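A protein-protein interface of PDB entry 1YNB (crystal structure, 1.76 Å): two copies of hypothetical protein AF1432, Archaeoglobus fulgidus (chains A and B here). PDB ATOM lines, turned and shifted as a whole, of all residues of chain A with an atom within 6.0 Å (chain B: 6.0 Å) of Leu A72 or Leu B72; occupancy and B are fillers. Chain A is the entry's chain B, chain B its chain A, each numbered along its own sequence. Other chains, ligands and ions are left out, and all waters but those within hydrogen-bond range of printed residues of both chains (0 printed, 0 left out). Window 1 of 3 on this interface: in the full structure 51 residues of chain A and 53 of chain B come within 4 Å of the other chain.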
ATOM      1  N   LEU A  20       7.962  -2.992   3.081  1.00  0.00           N
ATOM      2  CA  LEU A  20       9.071  -3.743   3.644  1.00  0.00           C
ATOM      3  C   LEU A  20      10.189  -3.948   2.625  1.00  0.00           C
ATOM      4  O   LEU A  20      11.306  -4.300   3.013  1.00  0.00           O
ATOM      5  CB  LEU A  20       8.602  -5.092   4.176  1.00  0.00           C
ATOM      6  CG  LEU A  20       7.708  -4.921   5.417  1.00  0.00           C
ATOM      7  CD1 LEU A  20       7.064  -6.270   5.787  1.00  0.00           C
ATOM      8  CD2 LEU A  20       8.544  -4.408   6.575  1.00  0.00           C
ATOM      9  N   ASN A  43      12.980 -11.640   5.477  1.00  0.00           N
ATOM     10  CA  ASN A  43      11.802 -12.520   5.667  1.00  0.00           C
ATOM     11  C   ASN A  43      11.694 -13.605   4.582  1.00  0.00           C
ATOM     12  O   ASN A  43      11.293 -14.746   4.860  1.00  0.00           O
ATOM     13  CB  ASN A  43      10.531 -11.718   5.638  1.00  0.00           C
ATOM     14  CG  ASN A  43      10.450 -10.711   6.753  1.00  0.00           C
ATOM     15  OD1 ASN A  43       9.777  -9.699   6.601  1.00  0.00           O
ATOM     16  ND2 ASN A  43      11.104 -10.978   7.875  1.00  0.00           N
ATOM     17  N   PHE A  44      11.968 -13.227   3.331  1.00  0.00           N
ATOM     18  CA  PHE A  44      11.966 -14.179   2.225  1.00  0.00           C
ATOM     19  C   PHE A  44      12.872 -15.342   2.543  1.00  0.00           C
ATOM     20  O   PHE A  44      12.442 -16.507   2.514  1.00  0.00           O
ATOM     21  CB  PHE A  44      12.478 -13.509   0.914  1.00  0.00           C
ATOM     22  CG  PHE A  44      12.795 -14.480  -0.210  1.00  0.00           C
ATOM     23  CD1 PHE A  44      11.755 -15.097  -0.933  1.00  0.00           C
ATOM     24  CD2 PHE A  44      14.119 -14.772  -0.548  1.00  0.00           C
ATOM     25  CE1 PHE A  44      12.035 -15.976  -1.949  1.00  0.00           C
ATOM     26  CE2 PHE A  44      14.414 -15.666  -1.580  1.00  0.00           C
ATOM     27  CZ  PHE A  44      13.349 -16.272  -2.279  1.00  0.00           C
ATOM     28  N   ALA A  47      11.937 -17.384   5.643  1.00  0.00           N
ATOM     29  CA  ALA A  47      10.780 -18.269   5.452  1.00  0.00           C
ATOM     30  C   ALA A  47      11.207 -19.583   4.808  1.00  0.00           C
ATOM     31  O   ALA A  47      10.771 -20.671   5.239  1.00  0.00           O
ATOM     32  CB  ALA A  47       9.680 -17.551   4.655  1.00  0.00           C
ATOM     33  N   ILE A  48      12.074 -19.525   3.797  1.00  0.00           N
ATOM     34  CA  ILE A  48      12.593 -20.720   3.162  1.00  0.00           C
ATOM     35  C   ILE A  48      13.410 -21.507   4.203  1.00  0.00           C
ATOM     36  O   ILE A  48      13.280 -22.743   4.327  1.00  0.00           O
ATOM     37  CB  ILE A  48      13.428 -20.328   1.902  1.00  0.00           C
ATOM     38  CG1 ILE A  48      12.453 -19.812   0.827  1.00  0.00           C
ATOM     39  CG2 ILE A  48      14.241 -21.505   1.349  1.00  0.00           C
ATOM     40  CD1 ILE A  48      13.147 -19.274  -0.406  1.00  0.00           C
ATOM     41  N   ALA A  67       5.375 -23.016   8.892  1.00  0.00           N
ATOM     42  CA  ALA A  67       6.506 -22.346   9.514  1.00  0.00           C
ATOM     43  C   ALA A  67       6.996 -21.281   8.517  1.00  0.00           C
ATOM     44  O   ALA A  67       7.346 -20.186   8.921  1.00  0.00           O
ATOM     45  CB  ALA A  67       7.607 -23.344   9.802  1.00  0.00           C
ATOM     46  N   ALA A  68       7.037 -21.615   7.247  1.00  0.00           N
ATOM     47  CA  ALA A  68       7.483 -20.623   6.258  1.00  0.00           C
ATOM     48  C   ALA A  68       6.562 -19.409   6.304  1.00  0.00           C
ATOM     49  O   ALA A  68       7.012 -18.272   6.419  1.00  0.00           O
ATOM     50  CB  ALA A  68       7.508 -21.227   4.863  1.00  0.00           C
ATOM     51  N   THR A  69       5.254 -19.649   6.274  1.00  0.00           N
ATOM     52  CA  THR A  69       4.297 -18.558   6.301  1.00  0.00           C
ATOM     53  C   THR A  69       4.413 -17.734   7.552  1.00  0.00           C
ATOM     54  O   THR A  69       4.345 -16.499   7.529  1.00  0.00           O
ATOM     55  CB  THR A  69       2.848 -19.126   6.148  1.00  0.00           C
ATOM     56  OG1 THR A  69       2.806 -19.943   4.976  1.00  0.00           O
ATOM     57  CG2 THR A  69       1.823 -18.016   6.057  1.00  0.00           C
ATOM     58  N   ALA A  70       4.584 -18.401   8.687  1.00  0.00           N
ATOM     59  CA  ALA A  70       4.710 -17.658   9.913  1.00  0.00           C
ATOM     60  C   ALA A  70       5.939 -16.741   9.878  1.00  0.00           C
ATOM     61  O   ALA A  70       5.905 -15.633  10.417  1.00  0.00           O
ATOM     62  CB  ALA A  70       4.822 -18.636  11.110  1.00  0.00           C
ATOM     63  N   ALA A  71       7.017 -17.214   9.277  1.00  0.00           N
ATOM     64  CA  ALA A  71       8.244 -16.402   9.179  1.00  0.00           C
ATOM     65  C   ALA A  71       8.000 -15.173   8.292  1.00  0.00           C
ATOM     66  O   ALA A  71       8.600 -14.115   8.520  1.00  0.00           O
ATOM     67  CB  ALA A  71       9.373 -17.220   8.598  1.00  0.00           C
ATOM     68  N   LEU A  72       7.135 -15.300   7.290  1.00  0.00           N
ATOM     69  CA  LEU A  72       6.832 -14.140   6.427  1.00  0.00           C
ATOM     70  C   LEU A  72       6.110 -13.044   7.189  1.00  0.00           C
ATOM     71  O   LEU A  72       6.287 -11.847   6.922  1.00  0.00           O
ATOM     72  CB  LEU A  72       5.944 -14.552   5.270  1.00  0.00           C
ATOM     73  CG  LEU A  72       6.508 -15.463   4.209  1.00  0.00           C
ATOM     74  CD1 LEU A  72       5.333 -15.870   3.292  1.00  0.00           C
ATOM     75  CD2 LEU A  72       7.602 -14.746   3.393  1.00  0.00           C
ATOM     76  N   PHE A  73       5.257 -13.436   8.135  1.00  0.00           N
ATOM     77  CA  PHE A  73       4.509 -12.475   8.923  1.00  0.00           C
ATOM     78  C   PHE A  73       5.271 -11.994  10.144  1.00  0.00           C
ATOM     79  O   PHE A  73       4.831 -11.063  10.821  1.00  0.00           O
ATOM     80  CB  PHE A  73       3.177 -13.094   9.385  1.00  0.00           C
ATOM     81  CG  PHE A  73       2.128 -13.140   8.316  1.00  0.00           C
ATOM     82  CD1 PHE A  73       1.225 -12.081   8.166  1.00  0.00           C
ATOM     83  CD2 PHE A  73       2.092 -14.184   7.405  1.00  0.00           C
ATOM     84  CE1 PHE A  73       0.301 -12.067   7.103  1.00  0.00           C
ATOM     85  CE2 PHE A  73       1.178 -14.195   6.339  1.00  0.00           C
ATOM     86  CZ  PHE A  73       0.280 -13.129   6.183  1.00  0.00           C
ATOM     87  N   HIS A  74       6.410 -12.620  10.419  1.00  0.00           N
ATOM     88  CA  HIS A  74       7.213 -12.337  11.602  1.00  0.00           C
ATOM     89  C   HIS A  74       7.542 -10.875  11.920  1.00  0.00           C
ATOM     90  O   HIS A  74       7.319 -10.411  13.039  1.00  0.00           O
ATOM     91  CB  HIS A  74       8.496 -13.173  11.534  1.00  0.00           C
ATOM     92  CG  HIS A  74       9.245 -13.239  12.828  1.00  0.00           C
ATOM     93  ND1 HIS A  74      10.624 -13.170  12.895  1.00  0.00           N
ATOM     94  CD2 HIS A  74       8.812 -13.394  14.102  1.00  0.00           C
ATOM     95  CE1 HIS A  74      11.004 -13.280  14.155  1.00  0.00           C
ATOM     96  NE2 HIS A  74       9.926 -13.416  14.907  1.00  0.00           N
ATOM     97  N   ASP A  75       8.063 -10.124  10.961  1.00  0.00           N
ATOM     98  CA  ASP A  75       8.378  -8.731  11.275  1.00  0.00           C
ATOM     99  C   ASP A  75       7.414  -7.798  10.593  1.00  0.00           C
ATOM    100  O   ASP A  75       7.727  -6.636  10.423  1.00  0.00           O
ATOM    101  CB  ASP A  75       9.801  -8.356  10.814  1.00  0.00           C
ATOM    102  CG  ASP A  75      10.851  -9.342  11.269  1.00  0.00           C
ATOM    103  OD1 ASP A  75      10.766  -9.838  12.425  1.00  0.00           O
ATOM    104  OD2 ASP A  75      11.776  -9.612  10.468  1.00  0.00           O
ATOM    105  N   LEU A  76       6.238  -8.288  10.206  1.00  0.00           N
ATOM    106  CA  LEU A  76       5.317  -7.446   9.480  1.00  0.00           C
ATOM    107  C   LEU A  76       5.059  -6.091  10.059  1.00  0.00           C
ATOM    108  O   LEU A  76       4.968  -5.102   9.317  1.00  0.00           O
ATOM    109  CB  LEU A  76       3.979  -8.140   9.262  1.00  0.00           C
ATOM    110  CG  LEU A  76       3.930  -9.022   8.023  1.00  0.00           C
ATOM    111  CD1 LEU A  76       2.457  -9.216   7.655  1.00  0.00           C
ATOM    112  CD2 LEU A  76       4.663  -8.367   6.834  1.00  0.00           C
ATOM    113  N   LEU B  20      18.988 -14.340  -4.568  1.00  0.00           N
ATOM    114  CA  LEU B  20      17.791 -13.711  -5.090  1.00  0.00           C
ATOM    115  C   LEU B  20      17.592 -12.306  -4.503  1.00  0.00           C
ATOM    116  O   LEU B  20      16.792 -11.530  -5.047  1.00  0.00           O
ATOM    117  CB  LEU B  20      16.549 -14.561  -4.827  1.00  0.00           C
ATOM    118  CG  LEU B  20      16.559 -15.829  -5.706  1.00  0.00           C
ATOM    119  CD1 LEU B  20      15.411 -16.725  -5.296  1.00  0.00           C
ATOM    120  CD2 LEU B  20      16.425 -15.441  -7.181  1.00  0.00           C
ATOM    121  N   ASN B  43       8.917 -12.178  -4.522  1.00  0.00           N
ATOM    122  CA  ASN B  43       8.430 -13.468  -3.949  1.00  0.00           C
ATOM    123  C   ASN B  43       7.853 -13.273  -2.553  1.00  0.00           C
ATOM    124  O   ASN B  43       6.861 -13.914  -2.162  1.00  0.00           O
ATOM    125  CB  ASN B  43       9.571 -14.461  -3.840  1.00  0.00           C
ATOM    126  CG  ASN B  43      10.149 -14.838  -5.177  1.00  0.00           C
ATOM    127  OD1 ASN B  43      11.338 -15.166  -5.270  1.00  0.00           O
ATOM    128  ND2 ASN B  43       9.322 -14.823  -6.219  1.00  0.00           N
ATOM    129  N   PHE B  44       8.507 -12.418  -1.774  1.00  0.00           N
ATOM    130  CA  PHE B  44       8.031 -12.106  -0.439  1.00  0.00           C
ATOM    131  C   PHE B  44       6.603 -11.630  -0.483  1.00  0.00           C
ATOM    132  O   PHE B  44       5.722 -12.194   0.186  1.00  0.00           O
ATOM    133  CB  PHE B  44       8.909 -10.999   0.207  1.00  0.00           C
ATOM    134  CG  PHE B  44       8.324 -10.397   1.464  1.00  0.00           C
ATOM    135  CD1 PHE B  44       8.326 -11.127   2.684  1.00  0.00           C
ATOM    136  CD2 PHE B  44       7.749  -9.112   1.448  1.00  0.00           C
ATOM    137  CE1 PHE B  44       7.772 -10.580   3.822  1.00  0.00           C
ATOM    138  CE2 PHE B  44       7.181  -8.555   2.613  1.00  0.00           C
ATOM    139  CZ  PHE B  44       7.197  -9.312   3.813  1.00  0.00           C
ATOM    140  N   ALA B  47       4.095 -14.094  -1.952  1.00  0.00           N
ATOM    141  CA  ALA B  47       3.740 -15.155  -0.992  1.00  0.00           C
ATOM    142  C   ALA B  47       2.648 -14.688  -0.066  1.00  0.00           C
ATOM    143  O   ALA B  47       1.664 -15.404   0.150  1.00  0.00           O
ATOM    144  CB  ALA B  47       4.986 -15.643  -0.226  1.00  0.00           C
ATOM    145  N   ILE B  48       2.764 -13.472   0.478  1.00  0.00           N
ATOM    146  CA  ILE B  48       1.729 -12.942   1.326  1.00  0.00           C
ATOM    147  C   ILE B  48       0.423 -12.797   0.522  1.00  0.00           C
ATOM    148  O   ILE B  48      -0.678 -13.146   0.996  1.00  0.00           O
ATOM    149  CB  ILE B  48       2.214 -11.610   1.957  1.00  0.00           C
ATOM    150  CG1 ILE B  48       3.362 -11.930   2.930  1.00  0.00           C
ATOM    151  CG2 ILE B  48       1.075 -10.864   2.693  1.00  0.00           C
ATOM    152  CD1 ILE B  48       4.050 -10.699   3.485  1.00  0.00           C
ATOM    153  N   ALA B  67       0.020 -22.181  -0.039  1.00  0.00           N
ATOM    154  CA  ALA B  67       0.023 -21.350  -1.227  1.00  0.00           C
ATOM    155  C   ALA B  67       1.159 -20.327  -1.072  1.00  0.00           C
ATOM    156  O   ALA B  67       1.849 -20.023  -2.038  1.00  0.00           O
ATOM    157  CB  ALA B  67      -1.318 -20.663  -1.366  1.00  0.00           C
ATOM    158  N   ALA B  68       1.301 -19.787   0.117  1.00  0.00           N
ATOM    159  CA  ALA B  68       2.365 -18.815   0.377  1.00  0.00           C
ATOM    160  C   ALA B  68       3.719 -19.461   0.166  1.00  0.00           C
ATOM    161  O   ALA B  68       4.596 -18.903  -0.502  1.00  0.00           O
ATOM    162  CB  ALA B  68       2.241 -18.266   1.778  1.00  0.00           C
ATOM    163  N   THR B  69       3.899 -20.674   0.696  1.00  0.00           N
ATOM    164  CA  THR B  69       5.171 -21.354   0.542  1.00  0.00           C
ATOM    165  C   THR B  69       5.484 -21.650  -0.900  1.00  0.00           C
ATOM    166  O   THR B  69       6.615 -21.481  -1.359  1.00  0.00           O
ATOM    167  CB  THR B  69       5.185 -22.685   1.366  1.00  0.00           C
ATOM    168  OG1 THR B  69       4.850 -22.385   2.712  1.00  0.00           O
ATOM    169  CG2 THR B  69       6.531 -23.330   1.317  1.00  0.00           C
ATOM    170  N   ALA B  70       4.480 -22.094  -1.644  1.00  0.00           N
ATOM    171  CA  ALA B  70       4.694 -22.397  -3.035  1.00  0.00           C
ATOM    172  C   ALA B  70       5.113 -21.134  -3.791  1.00  0.00           C
ATOM    173  O   ALA B  70       5.912 -21.194  -4.728  1.00  0.00           O
ATOM    174  CB  ALA B  70       3.386 -22.962  -3.648  1.00  0.00           C
ATOM    175  N   ALA B  71       4.553 -20.003  -3.398  1.00  0.00           N
ATOM    176  CA  ALA B  71       4.911 -18.731  -4.043  1.00  0.00           C
ATOM    177  C   ALA B  71       6.385 -18.415  -3.761  1.00  0.00           C
ATOM    178  O   ALA B  71       7.087 -17.860  -4.629  1.00  0.00           O
ATOM    179  CB  ALA B  71       4.031 -17.600  -3.498  1.00  0.00           C
ATOM    180  N   LEU B  72       6.871 -18.748  -2.565  1.00  0.00           N
ATOM    181  CA  LEU B  72       8.282 -18.476  -2.257  1.00  0.00           C
ATOM    182  C   LEU B  72       9.231 -19.245  -3.155  1.00  0.00           C
ATOM    183  O   LEU B  72      10.315 -18.753  -3.495  1.00  0.00           O
ATOM    184  CB  LEU B  72       8.598 -18.824  -0.814  1.00  0.00           C
ATOM    185  CG  LEU B  72       7.957 -17.960   0.249  1.00  0.00           C
ATOM    186  CD1 LEU B  72       8.199 -18.613   1.632  1.00  0.00           C
ATOM    187  CD2 LEU B  72       8.594 -16.551   0.196  1.00  0.00           C
ATOM    188  N   PHE B  73       8.854 -20.474  -3.522  1.00  0.00           N
ATOM    189  CA  PHE B  73       9.679 -21.315  -4.391  1.00  0.00           C
ATOM    190  C   PHE B  73       9.457 -21.083  -5.882  1.00  0.00           C
ATOM    191  O   PHE B  73      10.153 -21.671  -6.722  1.00  0.00           O
ATOM    192  CB  PHE B  73       9.407 -22.799  -4.088  1.00  0.00           C
ATOM    193  CG  PHE B  73      10.051 -23.283  -2.828  1.00  0.00           C
ATOM    194  CD1 PHE B  73      11.363 -23.781  -2.851  1.00  0.00           C
ATOM    195  CD2 PHE B  73       9.403 -23.158  -1.609  1.00  0.00           C
ATOM    196  CE1 PHE B  73      12.016 -24.143  -1.652  1.00  0.00           C
ATOM    197  CE2 PHE B  73      10.041 -23.518  -0.401  1.00  0.00           C
ATOM    198  CZ  PHE B  73      11.351 -24.007  -0.428  1.00  0.00           C
ATOM    199  N   HIS B  74       8.500 -20.231  -6.213  1.00  0.00           N
ATOM    200  CA  HIS B  74       8.132 -19.980  -7.595  1.00  0.00           C
ATOM    201  C   HIS B  74       9.244 -19.586  -8.565  1.00  0.00           C
ATOM    202  O   HIS B  74       9.376 -20.179  -9.630  1.00  0.00           O
ATOM    203  CB  HIS B  74       6.999 -18.953  -7.637  1.00  0.00           C
ATOM    204  CG  HIS B  74       6.296 -18.883  -8.956  1.00  0.00           C
ATOM    205  ND1 HIS B  74       5.726 -17.722  -9.437  1.00  0.00           N
ATOM    206  CD2 HIS B  74       6.047 -19.840  -9.882  1.00  0.00           C
ATOM    207  CE1 HIS B  74       5.156 -17.968 -10.604  1.00  0.00           C
ATOM    208  NE2 HIS B  74       5.337 -19.245 -10.896  1.00  0.00           N
ATOM    209  N   ASP B  75      10.070 -18.606  -8.232  1.00  0.00           N
ATOM    210  CA  ASP B  75      11.120 -18.254  -9.193  1.00  0.00           C
ATOM    211  C   ASP B  75      12.460 -18.698  -8.704  1.00  0.00           C
ATOM    212  O   ASP B  75      13.472 -18.227  -9.183  1.00  0.00           O
ATOM    213  CB  ASP B  75      11.168 -16.737  -9.411  1.00  0.00           C
ATOM    214  CG  ASP B  75       9.825 -16.163  -9.700  1.00  0.00           C
ATOM    215  OD1 ASP B  75       9.083 -16.778 -10.506  1.00  0.00           O
ATOM    216  OD2 ASP B  75       9.510 -15.102  -9.119  1.00  0.00           O
ATOM    217  N   LEU B  76      12.484 -19.634  -7.763  1.00  0.00           N
ATOM    218  CA  LEU B  76      13.743 -20.017  -7.193  1.00  0.00           C
ATOM    219  C   LEU B  76      14.838 -20.310  -8.191  1.00  0.00           C
ATOM    220  O   LEU B  76      15.998 -19.937  -7.984  1.00  0.00           O
ATOM    221  CB  LEU B  76      13.538 -21.192  -6.239  1.00  0.00           C
ATOM    222  CG  LEU B  76      14.243 -20.930  -4.911  1.00  0.00           C
ATOM    223  CD1 LEU B  76      13.832 -19.553  -4.362  1.00  0.00           C
ATOM    224  CD2 LEU B  76      13.887 -22.029  -3.907  1.00  0.00           C
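Among the printed residues, merely in contact across the chains: Phe A44 with Asn B43 (3.5 Å), Asn A43 with Phe B44 (3.5 Å), Ala A47 with Leu B72 (3.5 Å), Leu A72 with Ala B47 (3.5 Å), Ala A68 with Thr B69 (3.6 Å), Phe A44 with Leu B72 (3.6 Å), Leu A20 with Phe B44 (3.6 Å), Thr A69 with Ala B68 (3.7 Å), Leu A72 with Phe B44 (3.7 Å), Phe A44 with Leu B20 (3.7 Å), Leu A72 with Leu B72 (3.8 Å), Thr A69 with Thr B69 (3.9 Å) and Phe A44 with Leu B76 (3.9 Å).
Leu A20 touches Phe B44, and with the chains exchanged Phe A44 touches Leu B20. Phe A44 touches Leu B76, but with the chains exchanged Leu A76 does not touch Phe B44 (4.1 Å). Thr A69 touches its own counterpart, Thr B69. Leu A72 touches its own counterpart, Leu B72. Of the 13 pairs that touch across the chains among the printed residues, 12 have their exchanged pair printed and touching as well.
The side-chain amide nitrogen (ND2) of Asn B43 is in hydrogen-bond range of the side-chain carboxylate (OD2) of Asp B75 (2.9 Å). The side-chain amide nitrogen of Asn A43 lies within hydrogen-bond range of the side-chain carboxylate of Asp A75.
Of the 15 printed residues of chain A, 7 touch a printed residue of chain B. Hydrophobic or aromatic side chains of chain A that line the printed part of chain B: Leu A20, Phe A44, Ala A47, Ala A68 and Leu A72. Along chain A the printed residues that touch a printed residue of chain B span positions 20 to 72. Printed residues of chain B that touch a printed residue of chain A: Leu B20, Asn B43, Phe B44, Ala B47, Ala B68, Thr B69, Leu B72 and Leu B76. Hydrophobic or aromatic side chains of chain B within 4 Å of the printed part of chain A: Leu B20, Phe B44, Ala B47, Ala B68, Leu B72 and Leu B76. Among the printed residues, 13 pairs touch across the chains.
Leu B72 touches just these residues of chain A: Phe A44, Ala A47 and Leu A72. Printed residues of chain A within 4 Å of Thr B69: Ala A68 and Thr A69. Of the printed residues of chain A, Phe B44 touches Leu A20 (3.6 Å), Asn A43 (3.5 Å) and Leu A72 (3.7 Å). Of the printed residues of chain A, Ala B47 touches Leu A72 (3.5 Å). Printed residues of chain B within 4 Å of Asn A43: Phe B44. Of the printed residues of chain A, Asn B43 touches Phe A44 (3.5 Å). Asp A75 touches none of the printed residues of chain B. Phe A73 touches none of the printed residues of chain B. The nearest printed residue of chain A that does not touch Leu B72 is Ala A68 (4.2 Å).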
